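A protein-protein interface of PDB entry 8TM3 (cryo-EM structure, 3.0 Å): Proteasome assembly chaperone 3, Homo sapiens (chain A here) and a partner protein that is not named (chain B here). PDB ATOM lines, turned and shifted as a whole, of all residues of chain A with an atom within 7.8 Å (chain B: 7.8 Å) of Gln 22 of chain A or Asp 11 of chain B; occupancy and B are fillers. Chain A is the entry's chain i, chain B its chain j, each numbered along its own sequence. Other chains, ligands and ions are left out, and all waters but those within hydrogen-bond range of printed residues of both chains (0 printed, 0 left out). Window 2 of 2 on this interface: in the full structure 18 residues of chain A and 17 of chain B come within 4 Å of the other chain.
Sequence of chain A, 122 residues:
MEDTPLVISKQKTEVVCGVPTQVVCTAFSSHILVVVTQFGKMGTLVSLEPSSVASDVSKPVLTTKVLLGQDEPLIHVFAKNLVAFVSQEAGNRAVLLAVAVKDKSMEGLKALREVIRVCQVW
Hydrophobic or aromatic side chains of chain A that line the printed part of chain B: Val 24. Along chain A the printed residues that touch a printed residue of chain B span positions 11 to 41. Hydrophobic or aromatic side chains of chain B within 4 Å of the printed part of chain A: Val 12, Leu 14 and Leu 33. Among the printed residues, no Asp or Glu carboxylate lies within 4 Å of a Lys or Arg side-chain nitrogen of the other chain.
Of the printed residues of chain B, Gln 11 of chain A touches Leu 14. Gln 22 of chain A touches just these residues of chain B: Asp 11 and Val 12. Val 34 of chain A touches none of the printed residues of chain B. Asp 11 of chain B touches just one residue of chain A: Gln 22 (3.8 Å). Printed residues of chain A within 4 Å of Leu 14 of chain B: Gln 11 and Val 24. The nearest printed residue of chain B that does not touch Val 24 of chain A is Val 12 of chain B (4.7 Å).
The side-chain amide oxygen of Gln 22 of chain A is in hydrogen-bond range of the backbone NH of Val 12 of chain B, at 3.1 Å. The backbone carbonyl oxygen of Gly 40 of chain A lies within hydrogen-bond range of the backbone NH of Thr 34 of chain B, at 3.0 Å.
N of Thr 13 of chain A sits close to NE2 of Gln 11 of chain A (2.8 Å). The side-chain amide oxygen of Gln 11 of chain A lies close to the backbone carbonyl oxygen of Gln 22 of chain A, at 3.4 Å. The backbone carbonyl oxygen of Val 23 of chain A sits close to the side-chain amide oxygen of Gln 11 of chain A (2.6 Å). The backbone NH of Gln 22 of chain A is in hydrogen-bond range of the backbone carbonyl oxygen of Thr 37 of chain A (3.4 Å). The backbone carbonyl oxygen of Val 24 of chain A lies within hydrogen-bond range of the backbone NH of Val 35 of chain A (2.6 Å). The side-chain hydroxyl of Thr 37 of chain A sits at hydrogen-bond distance from the backbone carbonyl oxygen of Lys 41 of chain A (2.7 Å).
Among the printed residues, pairs that only touch across the chains: Gln 11 of chain A with Leu 14 of chain B (3.7 Å), Gln 22 of chain A with Asp 11 of chain B (3.8 Å), Val 24 of chain A with Leu 14 of chain B (3.3 Å), Gly 40 of chain A with Leu 33 of chain B (3.6 Å) and Lys 41 of chain A with Thr 34 of chain B (3.3 Å).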
ATOM      1  N   LYS A  10      20.161  -3.659   3.522  1.00  0.00           N
ATOM      2  CA  LYS A  10      19.600  -4.996   3.386  1.00  0.00           C
ATOM      3  C   LYS A  10      20.697  -6.017   3.646  1.00  0.00           C
ATOM      4  O   LYS A  10      21.777  -5.936   3.052  1.00  0.00           O
ATOM      5  CB  LYS A  10      18.996  -5.208   1.997  1.00  0.00           C
ATOM      6  N   GLN A  11      20.417  -6.974   4.527  1.00  0.00           N
ATOM      7  CA  GLN A  11      21.390  -7.978   4.934  1.00  0.00           C
ATOM      8  C   GLN A  11      20.803  -9.358   4.686  1.00  0.00           C
ATOM      9  O   GLN A  11      19.663  -9.629   5.078  1.00  0.00           O
ATOM     10  CB  GLN A  11      21.770  -7.795   6.412  1.00  0.00           C
ATOM     11  CG  GLN A  11      22.012  -9.080   7.201  1.00  0.00           C
ATOM     12  CD  GLN A  11      23.146  -9.914   6.635  1.00  0.00           C
ATOM     13  OE1 GLN A  11      24.099  -9.386   6.067  1.00  0.00           O
ATOM     14  NE2 GLN A  11      23.048 -11.225   6.798  1.00  0.00           N
ATOM     15  N   LYS A  12      21.580 -10.223   4.036  1.00  0.00           N
ATOM     16  CA  LYS A  12      21.157 -11.584   3.722  1.00  0.00           C
ATOM     17  C   LYS A  12      22.285 -12.537   4.094  1.00  0.00           C
ATOM     18  O   LYS A  12      23.321 -12.566   3.424  1.00  0.00           O
ATOM     19  CB  LYS A  12      20.797 -11.721   2.243  1.00  0.00           C
ATOM     20  N   THR A  13      22.083 -13.315   5.154  1.00  0.00           N
ATOM     21  CA  THR A  13      23.071 -14.293   5.600  1.00  0.00           C
ATOM     22  C   THR A  13      22.767 -15.626   4.926  1.00  0.00           C
ATOM     23  O   THR A  13      21.792 -16.300   5.273  1.00  0.00           O
ATOM     24  CB  THR A  13      23.071 -14.430   7.123  1.00  0.00           C
ATOM     25  OG1 THR A  13      23.840 -15.578   7.502  1.00  0.00           O
ATOM     26  CG2 THR A  13      21.652 -14.558   7.679  1.00  0.00           C
ATOM     27  N   GLU A  14      23.603 -16.004   3.963  1.00  0.00           N
ATOM     28  CA  GLU A  14      23.398 -17.209   3.173  1.00  0.00           C
ATOM     29  C   GLU A  14      24.683 -18.018   3.210  1.00  0.00           C
ATOM     30  O   GLU A  14      25.777 -17.457   3.086  1.00  0.00           O
ATOM     31  CB  GLU A  14      22.982 -16.839   1.735  1.00  0.00           C
ATOM     32  CG  GLU A  14      22.463 -17.979   0.847  1.00  0.00           C
ATOM     33  CD  GLU A  14      23.494 -19.044   0.526  1.00  0.00           C
ATOM     34  OE1 GLU A  14      23.105 -20.100  -0.017  1.00  0.00           O
ATOM     35  OE2 GLU A  14      24.695 -18.805   0.745  1.00  0.00           O
ATOM     36  N   VAL A  15      24.551 -19.333   3.378  1.00  0.00           N
ATOM     37  CA  VAL A  15      25.707 -20.225   3.511  1.00  0.00           C
ATOM     38  C   VAL A  15      25.953 -20.834   2.133  1.00  0.00           C
ATOM     39  O   VAL A  15      25.288 -21.782   1.713  1.00  0.00           O
ATOM     40  CB  VAL A  15      25.497 -21.286   4.592  1.00  0.00           C
ATOM     41  CG1 VAL A  15      25.450 -20.635   5.964  1.00  0.00           C
ATOM     42  CG2 VAL A  15      24.227 -22.106   4.343  1.00  0.00           C
ATOM     43  N   VAL A  19      30.619 -21.460   3.601  1.00  0.00           N
ATOM     44  CA  VAL A  19      30.967 -20.340   4.472  1.00  0.00           C
ATOM     45  C   VAL A  19      29.755 -19.424   4.626  1.00  0.00           C
ATOM     46  O   VAL A  19      29.174 -18.998   3.617  1.00  0.00           O
ATOM     47  CB  VAL A  19      32.185 -19.575   3.930  1.00  0.00           C
ATOM     48  CG1 VAL A  19      33.395 -20.496   3.859  1.00  0.00           C
ATOM     49  CG2 VAL A  19      31.893 -18.979   2.560  1.00  0.00           C
ATOM     50  N   PRO A  20      29.325 -19.099   5.858  1.00  0.00           N
ATOM     51  CA  PRO A  20      28.178 -18.172   6.033  1.00  0.00           C
ATOM     52  C   PRO A  20      28.526 -16.705   5.787  1.00  0.00           C
ATOM     53  O   PRO A  20      28.854 -15.931   6.686  1.00  0.00           O
ATOM     54  CB  PRO A  20      27.763 -18.418   7.488  1.00  0.00           C
ATOM     55  CG  PRO A  20      28.503 -19.635   7.941  1.00  0.00           C
ATOM     56  CD  PRO A  20      29.748 -19.676   7.142  1.00  0.00           C
ATOM     57  N   THR A  21      28.458 -16.298   4.523  1.00  0.00           N
ATOM     58  CA  THR A  21      28.728 -14.914   4.157  1.00  0.00           C
ATOM     59  C   THR A  21      27.521 -14.052   4.510  1.00  0.00           C
ATOM     60  O   THR A  21      26.416 -14.286   4.007  1.00  0.00           O
ATOM     61  CB  THR A  21      29.046 -14.796   2.668  1.00  0.00           C
ATOM     62  OG1 THR A  21      27.827 -14.758   1.917  1.00  0.00           O
ATOM     63  CG2 THR A  21      29.902 -15.963   2.199  1.00  0.00           C
ATOM     64  N   GLN A  22      27.732 -13.056   5.370  1.00  0.00           N
ATOM     65  CA  GLN A  22      26.677 -12.125   5.765  1.00  0.00           C
ATOM     66  C   GLN A  22      26.832 -10.853   4.935  1.00  0.00           C
ATOM     67  O   GLN A  22      27.374  -9.843   5.381  1.00  0.00           O
ATOM     68  CB  GLN A  22      26.742 -11.837   7.261  1.00  0.00           C
ATOM     69  CG  GLN A  22      27.202 -13.013   8.102  1.00  0.00           C
ATOM     70  CD  GLN A  22      26.865 -12.838   9.569  1.00  0.00           C
ATOM     71  OE1 GLN A  22      26.622 -11.725  10.034  1.00  0.00           O
ATOM     72  NE2 GLN A  22      26.850 -13.941  10.308  1.00  0.00           N
ATOM     73  N   VAL A  23      26.341 -10.914   3.700  1.00  0.00           N
ATOM     74  CA  VAL A  23      26.443  -9.776   2.796  1.00  0.00           C
ATOM     75  C   VAL A  23      25.533  -8.662   3.298  1.00  0.00           C
ATOM     76  O   VAL A  23      24.329  -8.864   3.494  1.00  0.00           O
ATOM     77  CB  VAL A  23      26.082 -10.184   1.362  1.00  0.00           C
ATOM     78  CG1 VAL A  23      26.144  -8.980   0.433  1.00  0.00           C
ATOM     79  CG2 VAL A  23      27.012 -11.285   0.881  1.00  0.00           C
ATOM     80  N   VAL A  24      26.109  -7.482   3.510  1.00  0.00           N
ATOM     81  CA  VAL A  24      25.372  -6.294   3.927  1.00  0.00           C
ATOM     82  C   VAL A  24      25.599  -5.211   2.884  1.00  0.00           C
ATOM     83  O   VAL A  24      26.717  -5.050   2.380  1.00  0.00           O
ATOM     84  CB  VAL A  24      25.809  -5.806   5.319  1.00  0.00           C
ATOM     85  CG1 VAL A  24      24.969  -4.615   5.745  1.00  0.00           C
ATOM     86  CG2 VAL A  24      25.713  -6.926   6.341  1.00  0.00           C
ATOM     87  N   CYS A  25      24.542  -4.472   2.558  1.00  0.00           N
ATOM     88  CA  CYS A  25      24.600  -3.408   1.559  1.00  0.00           C
ATOM     89  C   CYS A  25      23.870  -2.191   2.115  1.00  0.00           C
ATOM     90  O   CYS A  25      22.638  -2.137   2.097  1.00  0.00           O
ATOM     91  CB  CYS A  25      23.992  -3.869   0.240  1.00  0.00           C
ATOM     92  SG  CYS A  25      24.639  -5.452  -0.325  1.00  0.00           S
ATOM     93  N   VAL A  34      29.343  -2.217   0.719  1.00  0.00           N
ATOM     94  CA  VAL A  34      29.031  -3.624   0.491  1.00  0.00           C
ATOM     95  C   VAL A  34      29.908  -4.442   1.427  1.00  0.00           C
ATOM     96  O   VAL A  34      31.111  -4.593   1.191  1.00  0.00           O
ATOM     97  CB  VAL A  34      29.258  -4.019  -0.973  1.00  0.00           C
ATOM     98  CG1 VAL A  34      28.974  -5.499  -1.176  1.00  0.00           C
ATOM     99  CG2 VAL A  34      28.395  -3.169  -1.890  1.00  0.00           C
ATOM    100  N   VAL A  35      29.312  -4.986   2.486  1.00  0.00           N
ATOM    101  CA  VAL A  35      30.070  -5.711   3.498  1.00  0.00           C
ATOM    102  C   VAL A  35      29.866  -7.208   3.315  1.00  0.00           C
ATOM    103  O   VAL A  35      28.886  -7.778   3.809  1.00  0.00           O
ATOM    104  CB  VAL A  35      29.667  -5.275   4.918  1.00  0.00           C
ATOM    105  CG1 VAL A  35      30.668  -5.792   5.939  1.00  0.00           C
ATOM    106  CG2 VAL A  35      29.545  -3.761   4.997  1.00  0.00           C
ATOM    107  N   VAL A  36      30.790  -7.851   2.605  1.00  0.00           N
ATOM    108  CA  VAL A  36      30.801  -9.308   2.474  1.00  0.00           C
ATOM    109  C   VAL A  36      31.745  -9.813   3.561  1.00  0.00           C
ATOM    110  O   VAL A  36      32.953  -9.943   3.360  1.00  0.00           O
ATOM    111  CB  VAL A  36      31.227  -9.754   1.079  1.00  0.00           C
ATOM    112  CG1 VAL A  36      31.177 -11.267   0.964  1.00  0.00           C
ATOM    113  CG2 VAL A  36      30.343  -9.105   0.025  1.00  0.00           C
ATOM    114  N   THR A  37      31.184 -10.105   4.730  1.00  0.00           N
ATOM    115  CA  THR A  37      31.966 -10.439   5.915  1.00  0.00           C
ATOM    116  C   THR A  37      31.923 -11.945   6.143  1.00  0.00           C
ATOM    117  O   THR A  37      30.872 -12.504   6.470  1.00  0.00           O
ATOM    118  CB  THR A  37      31.453  -9.689   7.145  1.00  0.00           C
ATOM    119  OG1 THR A  37      32.024 -10.261   8.329  1.00  0.00           O
ATOM    120  CG2 THR A  37      29.930  -9.746   7.238  1.00  0.00           C
ATOM    121  N   GLN A  38      33.064 -12.596   5.963  1.00  0.00           N
ATOM    122  CA  GLN A  38      33.273 -13.960   6.418  1.00  0.00           C
ATOM    123  C   GLN A  38      34.081 -13.931   7.709  1.00  0.00           C
ATOM    124  O   GLN A  38      34.766 -12.952   8.019  1.00  0.00           O
ATOM    125  CB  GLN A  38      33.988 -14.792   5.350  1.00  0.00           C
ATOM    126  CG  GLN A  38      33.931 -16.288   5.590  1.00  0.00           C
ATOM    127  CD  GLN A  38      34.486 -17.082   4.427  1.00  0.00           C
ATOM    128  OE1 GLN A  38      34.205 -16.783   3.266  1.00  0.00           O
ATOM    129  NE2 GLN A  38      35.285 -18.097   4.732  1.00  0.00           N
ATOM    130  N   PHE A  39      33.987 -15.014   8.473  1.00  0.00           N
ATOM    131  CA  PHE A  39      34.475 -15.075   9.847  1.00  0.00           C
ATOM    132  C   PHE A  39      33.815 -14.031  10.740  1.00  0.00           C
ATOM    133  O   PHE A  39      34.304 -13.771  11.845  1.00  0.00           O
ATOM    134  CB  PHE A  39      36.001 -14.916   9.929  1.00  0.00           C
ATOM    135  CG  PHE A  39      36.742 -15.421   8.722  1.00  0.00           C
ATOM    136  CD1 PHE A  39      37.002 -16.773   8.570  1.00  0.00           C
ATOM    137  CD2 PHE A  39      37.189 -14.547   7.749  1.00  0.00           C
ATOM    138  CE1 PHE A  39      37.688 -17.239   7.465  1.00  0.00           C
ATOM    139  CE2 PHE A  39      37.875 -15.009   6.644  1.00  0.00           C
ATOM    140  CZ  PHE A  39      38.125 -16.356   6.502  1.00  0.00           C
ATOM    141  N   GLY A  40      32.722 -13.422  10.290  1.00  0.00           N
ATOM    142  CA  GLY A  40      32.036 -12.422  11.092  1.00  0.00           C
ATOM    143  C   GLY A  40      32.897 -11.234  11.459  1.00  0.00           C
ATOM    144  O   GLY A  40      32.806 -10.731  12.586  1.00  0.00           O
ATOM    145  N   LYS A  41      33.730 -10.767  10.531  1.00  0.00           N
ATOM    146  CA  LYS A  41      34.613  -9.638  10.788  1.00  0.00           C
ATOM    147  C   LYS A  41      34.744  -8.798   9.526  1.00  0.00           C
ATOM    148  O   LYS A  41      34.478  -9.259   8.414  1.00  0.00           O
ATOM    149  CB  LYS A  41      35.996 -10.098  11.267  1.00  0.00           C
ATOM    150  CG  LYS A  41      36.013 -10.586  12.707  1.00  0.00           C
ATOM    151  CD  LYS A  41      37.197 -11.496  12.982  1.00  0.00           C
ATOM    152  CE  LYS A  41      37.069 -12.177  14.334  1.00  0.00           C
ATOM    153  NZ  LYS A  41      38.143 -13.183  14.557  1.00  0.00           N
ATOM    154  N   ALA A  98      33.872  -4.216   1.848  1.00  0.00           N
ATOM    155  CA  ALA A  98      34.619  -4.796   2.963  1.00  0.00           C
ATOM    156  C   ALA A  98      34.576  -6.315   2.826  1.00  0.00           C
ATOM    157  O   ALA A  98      33.857  -7.015   3.540  1.00  0.00           O
ATOM    158  CB  ALA A  98      34.044  -4.328   4.294  1.00  0.00           C
ATOM    159  N   LEU A 112      28.587 -15.112  -4.408  1.00  0.00           N
ATOM    160  CA  LEU A 112      28.480 -13.849  -3.689  1.00  0.00           C
ATOM    161  C   LEU A 112      27.757 -12.803  -4.526  1.00  0.00           C
ATOM    162  O   LEU A 112      27.000 -11.990  -3.991  1.00  0.00           O
ATOM    163  CB  LEU A 112      29.862 -13.347  -3.279  1.00  0.00           C
ATOM    164  CG  LEU A 112      30.792 -14.345  -2.587  1.00  0.00           C
ATOM    165  CD1 LEU A 112      31.967 -13.623  -1.971  1.00  0.00           C
ATOM    166  CD2 LEU A 112      30.052 -15.160  -1.534  1.00  0.00           C
ATOM    167  N   VAL A 115      24.176 -13.439  -4.208  1.00  0.00           N
ATOM    168  CA  VAL A 115      23.743 -13.093  -2.854  1.00  0.00           C
ATOM    169  C   VAL A 115      23.544 -11.586  -2.722  1.00  0.00           C
ATOM    170  O   VAL A 115      22.540 -11.125  -2.163  1.00  0.00           O
ATOM    171  CB  VAL A 115      24.750 -13.622  -1.817  1.00  0.00           C
ATOM    172  CG1 VAL A 115      24.455 -13.035  -0.446  1.00  0.00           C
ATOM    173  CG2 VAL A 115      24.695 -15.136  -1.756  1.00  0.00           C
ATOM    174  N   CYS A 119      20.290  -9.290  -1.817  1.00  0.00           N
ATOM    175  CA  CYS A 119      20.247  -8.283  -0.763  1.00  0.00           C
ATOM    176  C   CYS A 119      20.439  -6.871  -1.304  1.00  0.00           C
ATOM    177  O   CYS A 119      21.012  -6.016  -0.621  1.00  0.00           O
ATOM    178  CB  CYS A 119      21.302  -8.590   0.300  1.00  0.00           C
ATOM    179  N   ASP B  11      25.839 -12.743  15.021  1.00  0.00           N
ATOM    180  CA  ASP B  11      25.669 -12.222  13.635  1.00  0.00           C
ATOM    181  C   ASP B  11      25.719 -10.699  13.621  1.00  0.00           C
ATOM    182  O   ASP B  11      25.890 -10.065  14.661  1.00  0.00           O
ATOM    183  CB  ASP B  11      24.348 -12.710  13.037  1.00  0.00           C
ATOM    184  N   VAL B  12      25.566 -10.119  12.436  1.00  0.00           N
ATOM    185  CA  VAL B  12      25.626  -8.673  12.260  1.00  0.00           C
ATOM    186  C   VAL B  12      24.241  -8.106  12.548  1.00  0.00           C
ATOM    187  O   VAL B  12      23.279  -8.397  11.833  1.00  0.00           O
ATOM    188  CB  VAL B  12      26.098  -8.298  10.851  1.00  0.00           C
ATOM    189  N   SER B  13      24.141  -7.296  13.598  1.00  0.00           N
ATOM    190  CA  SER B  13      22.893  -6.632  13.961  1.00  0.00           C
ATOM    191  C   SER B  13      22.943  -5.202  13.439  1.00  0.00           C
ATOM    192  O   SER B  13      23.688  -4.367  13.963  1.00  0.00           O
ATOM    193  CB  SER B  13      22.687  -6.662  15.473  1.00  0.00           C
ATOM    194  N   LEU B  14      22.147  -4.917  12.408  1.00  0.00           N
ATOM    195  CA  LEU B  14      22.137  -3.601  11.772  1.00  0.00           C
ATOM    196  C   LEU B  14      21.162  -2.704  12.528  1.00  0.00           C
ATOM    197  O   LEU B  14      20.015  -2.491  12.128  1.00  0.00           O
ATOM    198  CB  LEU B  14      21.769  -3.719  10.299  1.00  0.00           C
ATOM    199  CG  LEU B  14      22.663  -4.619   9.441  1.00  0.00           C
ATOM    200  CD1 LEU B  14      22.309  -6.092   9.614  1.00  0.00           C
ATOM    201  CD2 LEU B  14      22.556  -4.211   7.983  1.00  0.00           C
ATOM    202  N   MET B  31      26.912  -1.686  12.624  1.00  0.00           N
ATOM    203  CA  MET B  31      27.146  -3.008  12.048  1.00  0.00           C
ATOM    204  C   MET B  31      27.988  -3.794  13.043  1.00  0.00           C
ATOM    205  O   MET B  31      29.203  -3.593  13.128  1.00  0.00           O
ATOM    206  CB  MET B  31      27.844  -2.909  10.691  1.00  0.00           C
ATOM    207  N   ARG B  32      27.343  -4.690  13.791  1.00  0.00           N
ATOM    208  CA  ARG B  32      28.018  -5.332  14.915  1.00  0.00           C
ATOM    209  C   ARG B  32      29.106  -6.293  14.451  1.00  0.00           C
ATOM    210  O   ARG B  32      30.204  -6.312  15.020  1.00  0.00           O
ATOM    211  CB  ARG B  32      26.999  -6.071  15.781  1.00  0.00           C
ATOM    212  CG  ARG B  32      26.036  -5.155  16.519  1.00  0.00           C
ATOM    213  CD  ARG B  32      26.687  -4.488  17.723  1.00  0.00           C
ATOM    214  NE  ARG B  32      27.413  -5.432  18.563  1.00  0.00           N
ATOM    215  CZ  ARG B  32      26.839  -6.343  19.337  1.00  0.00           C
ATOM    216  NH1 ARG B  32      25.523  -6.468  19.402  1.00  0.00           N
ATOM    217  NH2 ARG B  32      27.604  -7.152  20.064  1.00  0.00           N
ATOM    218  N   LEU B  33      28.826  -7.095  13.427  1.00  0.00           N
ATOM    219  CA  LEU B  33      29.728  -8.180  13.061  1.00  0.00           C
ATOM    220  C   LEU B  33      29.936  -9.079  14.275  1.00  0.00           C
ATOM    221  O   LEU B  33      28.961  -9.567  14.855  1.00  0.00           O
ATOM    222  CB  LEU B  33      31.057  -7.622  12.545  1.00  0.00           C
ATOM    223  N   THR B  34      31.188  -9.304  14.676  1.00  0.00           N
ATOM    224  CA  THR B  34      31.491 -10.014  15.912  1.00  0.00           C
ATOM    225  C   THR B  34      32.084  -9.075  16.954  1.00  0.00           C
ATOM    226  O   THR B  34      31.544  -8.947  18.056  1.00  0.00           O
ATOM    227  CB  THR B  34      32.457 -11.176  15.641  1.00  0.00           C
ATOM    228  OG1 THR B  34      33.522 -10.732  14.792  1.00  0.00           O
ATOM    229  CG2 THR B  34      31.729 -12.334  14.977  1.00  0.00           C
ATOM    230  N   ASP B  35      33.188  -8.407  16.622  1.00  0.00           N
ATOM    231  CA  ASP B  35      33.742  -7.352  17.455  1.00  0.00           C
ATOM    232  C   ASP B  35      34.088  -6.101  16.666  1.00  0.00           C
ATOM    233  O   ASP B  35      34.353  -5.061  17.279  1.00  0.00           O
ATOM    234  CB  ASP B  35      35.004  -7.840  18.183  1.00  0.00           C
ATOM    235  CG  ASP B  35      34.863  -9.252  18.716  1.00  0.00           C
ATOM    236  OD1 ASP B  35      33.765  -9.606  19.190  1.00  0.00           O
ATOM    237  OD2 ASP B  35      35.854 -10.008  18.661  1.00  0.00           O
